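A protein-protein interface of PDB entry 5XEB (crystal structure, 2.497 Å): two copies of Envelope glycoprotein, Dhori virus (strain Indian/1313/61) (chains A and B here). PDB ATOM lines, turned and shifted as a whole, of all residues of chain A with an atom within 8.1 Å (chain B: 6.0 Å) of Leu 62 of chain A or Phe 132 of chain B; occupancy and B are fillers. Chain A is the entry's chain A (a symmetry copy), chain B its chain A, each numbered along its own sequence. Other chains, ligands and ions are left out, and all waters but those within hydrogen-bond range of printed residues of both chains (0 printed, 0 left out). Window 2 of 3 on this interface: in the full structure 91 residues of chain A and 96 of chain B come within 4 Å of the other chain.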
ATOM      1  N   GLY A  59      -3.122   5.853 -20.999  1.00  0.00           N
ATOM      2  CA  GLY A  59      -3.127   4.719 -21.903  1.00  0.00           C
ATOM      3  C   GLY A  59      -3.995   3.559 -21.471  1.00  0.00           C
ATOM      4  O   GLY A  59      -3.928   2.492 -22.098  1.00  0.00           O
ATOM      5  N   GLY A  60      -4.809   3.719 -20.437  1.00  0.00           N
ATOM      6  CA  GLY A  60      -5.643   2.653 -19.928  1.00  0.00           C
ATOM      7  C   GLY A  60      -5.009   1.951 -18.739  1.00  0.00           C
ATOM      8  O   GLY A  60      -3.810   2.057 -18.477  1.00  0.00           O
ATOM      9  N   SER A  61      -5.847   1.215 -18.006  1.00  0.00           N
ATOM     10  CA  SER A  61      -5.360   0.421 -16.885  1.00  0.00           C
ATOM     11  C   SER A  61      -4.337  -0.619 -17.320  1.00  0.00           C
ATOM     12  O   SER A  61      -3.556  -1.094 -16.489  1.00  0.00           O
ATOM     13  CB  SER A  61      -6.534  -0.267 -16.188  1.00  0.00           C
ATOM     14  OG  SER A  61      -7.528   0.672 -15.815  1.00  0.00           O
ATOM     15  N   LEU A  62      -4.318  -0.974 -18.605  1.00  0.00           N
ATOM     16  CA  LEU A  62      -3.417  -2.009 -19.095  1.00  0.00           C
ATOM     17  C   LEU A  62      -2.031  -1.460 -19.408  1.00  0.00           C
ATOM     18  O   LEU A  62      -1.038  -2.186 -19.276  1.00  0.00           O
ATOM     19  CB  LEU A  62      -4.008  -2.675 -20.340  1.00  0.00           C
ATOM     20  CG  LEU A  62      -5.111  -3.734 -20.201  1.00  0.00           C
ATOM     21  CD1 LEU A  62      -6.307  -3.244 -19.396  1.00  0.00           C
ATOM     22  CD2 LEU A  62      -5.562  -4.200 -21.578  1.00  0.00           C
ATOM     23  N   ASP A  63      -1.940  -0.198 -19.819  1.00  0.00           N
ATOM     24  CA  ASP A  63      -0.663   0.392 -20.197  1.00  0.00           C
ATOM     25  C   ASP A  63       0.138   0.744 -18.947  1.00  0.00           C
ATOM     26  O   ASP A  63      -0.366   1.422 -18.047  1.00  0.00           O
ATOM     27  CB  ASP A  63      -0.891   1.636 -21.055  1.00  0.00           C
ATOM     28  CG  ASP A  63       0.349   2.054 -21.829  1.00  0.00           C
ATOM     29  OD1 ASP A  63       1.467   1.651 -21.444  1.00  0.00           O
ATOM     30  OD2 ASP A  63       0.206   2.794 -22.824  1.00  0.00           O
ATOM     31  N   LYS A  64       1.390   0.280 -18.895  1.00  0.00           N
ATOM     32  CA  LYS A  64       2.256   0.600 -17.766  1.00  0.00           C
ATOM     33  C   LYS A  64       2.688   2.062 -17.750  1.00  0.00           C
ATOM     34  O   LYS A  64       3.169   2.536 -16.717  1.00  0.00           O
ATOM     35  CB  LYS A  64       3.497  -0.294 -17.771  1.00  0.00           C
ATOM     36  CG  LYS A  64       3.313  -1.621 -17.059  1.00  0.00           C
ATOM     37  CD  LYS A  64       4.630  -2.379 -16.967  1.00  0.00           C
ATOM     38  CE  LYS A  64       4.456  -3.730 -16.284  1.00  0.00           C
ATOM     39  NZ  LYS A  64       5.723  -4.517 -16.281  1.00  0.00           N
ATOM     40  N   ASN A  65       2.545   2.776 -18.869  1.00  0.00           N
ATOM     41  CA  ASN A  65       2.882   4.191 -18.932  1.00  0.00           C
ATOM     42  C   ASN A  65       1.761   5.094 -18.438  1.00  0.00           C
ATOM     43  O   ASN A  65       1.971   6.306 -18.306  1.00  0.00           O
ATOM     44  CB  ASN A  65       3.259   4.580 -20.366  1.00  0.00           C
ATOM     45  CG  ASN A  65       4.470   3.826 -20.872  1.00  0.00           C
ATOM     46  OD1 ASN A  65       5.306   3.379 -20.089  1.00  0.00           O
ATOM     47  ND2 ASN A  65       4.572   3.678 -22.189  1.00  0.00           N
ATOM     48  N   THR A  66       0.582   4.543 -18.165  1.00  0.00           N
ATOM     49  CA  THR A  66      -0.522   5.338 -17.642  1.00  0.00           C
ATOM     50  C   THR A  66      -0.192   5.822 -16.235  1.00  0.00           C
ATOM     51  O   THR A  66       0.266   5.049 -15.392  1.00  0.00           O
ATOM     52  CB  THR A  66      -1.809   4.514 -17.621  1.00  0.00           C
ATOM     53  OG1 THR A  66      -2.117   4.073 -18.949  1.00  0.00           O
ATOM     54  CG2 THR A  66      -2.965   5.340 -17.085  1.00  0.00           C
ATOM     55  N   PHE A 132      -7.813  10.076 -23.220  1.00  0.00           N
ATOM     56  CA  PHE A 132      -7.336   8.734 -23.536  1.00  0.00           C
ATOM     57  C   PHE A 132      -6.323   8.761 -24.675  1.00  0.00           C
ATOM     58  O   PHE A 132      -6.465   9.520 -25.637  1.00  0.00           O
ATOM     59  CB  PHE A 132      -8.515   7.833 -23.905  1.00  0.00           C
ATOM     60  CG  PHE A 132      -8.119   6.428 -24.270  1.00  0.00           C
ATOM     61  CD1 PHE A 132      -7.907   5.480 -23.287  1.00  0.00           C
ATOM     62  CD2 PHE A 132      -7.973   6.053 -25.597  1.00  0.00           C
ATOM     63  CE1 PHE A 132      -7.542   4.186 -23.613  1.00  0.00           C
ATOM     64  CE2 PHE A 132      -7.611   4.759 -25.931  1.00  0.00           C
ATOM     65  CZ  PHE A 132      -7.398   3.825 -24.937  1.00  0.00           C
ATOM     66  N   ASN B  58      -4.557  -2.728  -9.137  1.00  0.00           N
ATOM     67  CA  ASN B  58      -4.981  -2.298 -10.468  1.00  0.00           C
ATOM     68  C   ASN B  58      -5.767  -3.429 -11.128  1.00  0.00           C
ATOM     69  O   ASN B  58      -5.189  -4.304 -11.777  1.00  0.00           O
ATOM     70  CB  ASN B  58      -3.773  -1.884 -11.310  1.00  0.00           C
ATOM     71  CG  ASN B  58      -4.169  -1.170 -12.586  1.00  0.00           C
ATOM     72  OD1 ASN B  58      -5.342  -0.864 -12.802  1.00  0.00           O
ATOM     73  ND2 ASN B  58      -3.190  -0.898 -13.440  1.00  0.00           N
ATOM     74  N   GLY B  59      -7.089  -3.403 -10.966  1.00  0.00           N
ATOM     75  CA  GLY B  59      -7.968  -4.354 -11.618  1.00  0.00           C
ATOM     76  C   GLY B  59      -8.833  -3.780 -12.716  1.00  0.00           C
ATOM     77  O   GLY B  59      -9.726  -4.482 -13.209  1.00  0.00           O
ATOM     78  N   GLY B  60      -8.606  -2.539 -13.127  1.00  0.00           N
ATOM     79  CA  GLY B  60      -9.409  -1.892 -14.140  1.00  0.00           C
ATOM     80  C   GLY B  60     -10.487  -1.011 -13.537  1.00  0.00           C
ATOM     81  O   GLY B  60     -10.836  -1.112 -12.359  1.00  0.00           O
ATOM     82  N   ASN B 129       0.326   2.778  -9.432  1.00  0.00           N
ATOM     83  CA  ASN B 129      -0.680   1.727  -9.554  1.00  0.00           C
ATOM     84  C   ASN B 129      -0.806   1.290 -11.011  1.00  0.00           C
ATOM     85  O   ASN B 129      -1.914   1.099 -11.525  1.00  0.00           O
ATOM     86  CB  ASN B 129      -2.032   2.196  -9.007  1.00  0.00           C
ATOM     87  CG  ASN B 129      -3.024   1.063  -8.826  1.00  0.00           C
ATOM     88  OD1 ASN B 129      -2.647  -0.108  -8.784  1.00  0.00           O
ATOM     89  ND2 ASN B 129      -4.301   1.411  -8.712  1.00  0.00           N
ATOM     90  N   ASN B 130       0.328   1.118 -11.690  1.00  0.00           N
ATOM     91  CA  ASN B 130       0.351   0.937 -13.136  1.00  0.00           C
ATOM     92  C   ASN B 130       0.611  -0.507 -13.556  1.00  0.00           C
ATOM     93  O   ASN B 130       0.938  -0.751 -14.722  1.00  0.00           O
ATOM     94  CB  ASN B 130       1.400   1.856 -13.760  1.00  0.00           C
ATOM     95  CG  ASN B 130       2.806   1.530 -13.299  1.00  0.00           C
ATOM     96  OD1 ASN B 130       3.004   0.996 -12.207  1.00  0.00           O
ATOM     97  ND2 ASN B 130       3.793   1.850 -14.129  1.00  0.00           N
ATOM     98  N   HIS B 131       0.474  -1.464 -12.644  1.00  0.00           N
ATOM     99  CA  HIS B 131       0.699  -2.877 -12.945  1.00  0.00           C
ATOM    100  C   HIS B 131      -0.655  -3.583 -12.951  1.00  0.00           C
ATOM    101  O   HIS B 131      -1.174  -3.959 -11.896  1.00  0.00           O
ATOM    102  CB  HIS B 131       1.666  -3.497 -11.942  1.00  0.00           C
ATOM    103  CG  HIS B 131       3.024  -2.867 -11.950  1.00  0.00           C
ATOM    104  ND1 HIS B 131       3.903  -3.008 -13.003  1.00  0.00           N
ATOM    105  CD2 HIS B 131       3.651  -2.083 -11.041  1.00  0.00           C
ATOM    106  CE1 HIS B 131       5.014  -2.343 -12.741  1.00  0.00           C
ATOM    107  NE2 HIS B 131       4.887  -1.773 -11.555  1.00  0.00           N
ATOM    108  N   PHE B 132      -1.214  -3.761 -14.149  1.00  0.00           N
ATOM    109  CA  PHE B 132      -2.555  -4.315 -14.299  1.00  0.00           C
ATOM    110  C   PHE B 132      -2.656  -5.699 -13.669  1.00  0.00           C
ATOM    111  O   PHE B 132      -1.729  -6.508 -13.755  1.00  0.00           O
ATOM    112  CB  PHE B 132      -2.929  -4.386 -15.781  1.00  0.00           C
ATOM    113  CG  PHE B 132      -4.292  -4.968 -16.040  1.00  0.00           C
ATOM    114  CD1 PHE B 132      -5.421  -4.175 -15.956  1.00  0.00           C
ATOM    115  CD2 PHE B 132      -4.442  -6.303 -16.380  1.00  0.00           C
ATOM    116  CE1 PHE B 132      -6.679  -4.700 -16.191  1.00  0.00           C
ATOM    117  CE2 PHE B 132      -5.697  -6.835 -16.620  1.00  0.00           C
ATOM    118  CZ  PHE B 132      -6.816  -6.032 -16.527  1.00  0.00           C
ATOM    119  N   ALA B 133      -3.799  -5.962 -13.033  1.00  0.00           N
ATOM    120  CA  ALA B 133      -4.099  -7.228 -12.365  1.00  0.00           C
ATOM    121  C   ALA B 133      -3.126  -7.540 -11.233  1.00  0.00           C
ATOM    122  O   ALA B 133      -2.986  -8.700 -10.835  1.00  0.00           O
ATOM    123  CB  ALA B 133      -4.135  -8.393 -13.363  1.00  0.00           C
ATOM    124  N   TYR B 134      -2.453  -6.525 -10.693  1.00  0.00           N
ATOM    125  CA  TYR B 134      -1.496  -6.724  -9.615  1.00  0.00           C
ATOM    126  C   TYR B 134      -1.664  -5.636  -8.565  1.00  0.00           C
ATOM    127  O   TYR B 134      -2.290  -4.596  -8.799  1.00  0.00           O
ATOM    128  CB  TYR B 134      -0.044  -6.729 -10.124  1.00  0.00           C
ATOM    129  CG  TYR B 134       0.314  -7.900 -11.014  1.00  0.00           C
ATOM    130  CD1 TYR B 134       0.348  -9.195 -10.514  1.00  0.00           C
ATOM    131  CD2 TYR B 134       0.640  -7.707 -12.350  1.00  0.00           C
ATOM    132  CE1 TYR B 134       0.681 -10.266 -11.325  1.00  0.00           C
ATOM    133  CE2 TYR B 134       0.972  -8.770 -13.167  1.00  0.00           C
ATOM    134  CZ  TYR B 134       0.991 -10.046 -12.650  1.00  0.00           C
ATOM    135  OH  TYR B 134       1.323 -11.107 -13.461  1.00  0.00           O
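The backbone carbonyl oxygen (O) of Ser 61 of chain A is in hydrogen-bond range of the side-chain amide nitrogen (ND2) of Asn 58 of chain B (3.1 Å). The backbone carbonyl oxygen (O) of Lys 64 of chain A lies within hydrogen-bond range of the side-chain amide nitrogen (ND2) of Asn 130 of chain B (2.7 Å).
NE2 of His 131 of chain B lies close to OD1 of Asn 130 of chain B (3.4 Å). ND2 of Asn 58 of chain B sits at hydrogen-bond distance from O of Asn 129 of chain B (3.0 Å). The backbone NH (N) of Ala 133 of chain B is in hydrogen-bond range of the backbone carbonyl oxygen (O) of Asn 58 of chain B, 2.5 Å away. The backbone NH (N) of Asn 58 of chain B sits at hydrogen-bond distance from the backbone carbonyl oxygen (O) of Tyr 134 of chain B (3.0 Å). The backbone carbonyl oxygen of Gly 60 of chain A is in hydrogen-bond range of the side-chain hydroxyl of Thr 66 of chain A, 2.7 Å away. The backbone NH (N) of Gly 59 of chain A is in hydrogen-bond range of the side-chain hydroxyl (OG1) of Thr 66 of chain A.
Ser 61 of chain A touches Gly 60 of chain B (OG to CA, 3.6 Å). CB of Phe 132 of chain B touches O of Ser 61 of chain A (3.4 Å). Phe 132 of chain B touches Leu 62 of chain A. CE of Lys 64 of chain A touches ND1 of His 131 of chain B, at 3.4 Å. Thr 66 of chain A touches Asn 130 of chain B.
Of chain B, only Phe 132 (3.5 Å) comes within 4 Å of Leu 62 of chain A. Printed residues of chain A within 4 Å of Gly 60 of chain B: Ser 61. Of the printed residues of chain A, Asn 130 of chain B touches Lys 64 (2.7 Å) and Thr 66 (3.8 Å). Of the printed residues of chain A, His 131 of chain B touches Lys 64. Printed residues of chain A within 4 Å of Phe 132 of chain B: Ser 61 and Leu 62. No residue of chain A comes within 4 Å of Ala 133 of chain B. The nearest residue of chain B that does not touch Leu 62 of chain A is Asn 130 of chain B (5.2 Å). The nearest residue of chain A that does not touch Phe 132 of chain B is Lys 64 of chain A (5.8 Å).
Of the 9 printed residues of chain A, 4 touch a printed residue of chain B. Printed residues of chain A that touch a printed residue of chain B: Ser 61, Leu 62, Lys 64 and Thr 66. Along chain A the printed residues that touch a printed residue of chain B span positions 61 to 66. Among the printed residues, 7 pairs touch across the chains. Among the printed residues, no Asp or Glu carboxylate lies within 4 Å of a Lys or Arg side-chain nitrogen of the other chain.
3 positions are printed for both chains. Of the 7 pairs that touch across the chains among the printed residues, none has its exchanged pair printed and touching as well.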
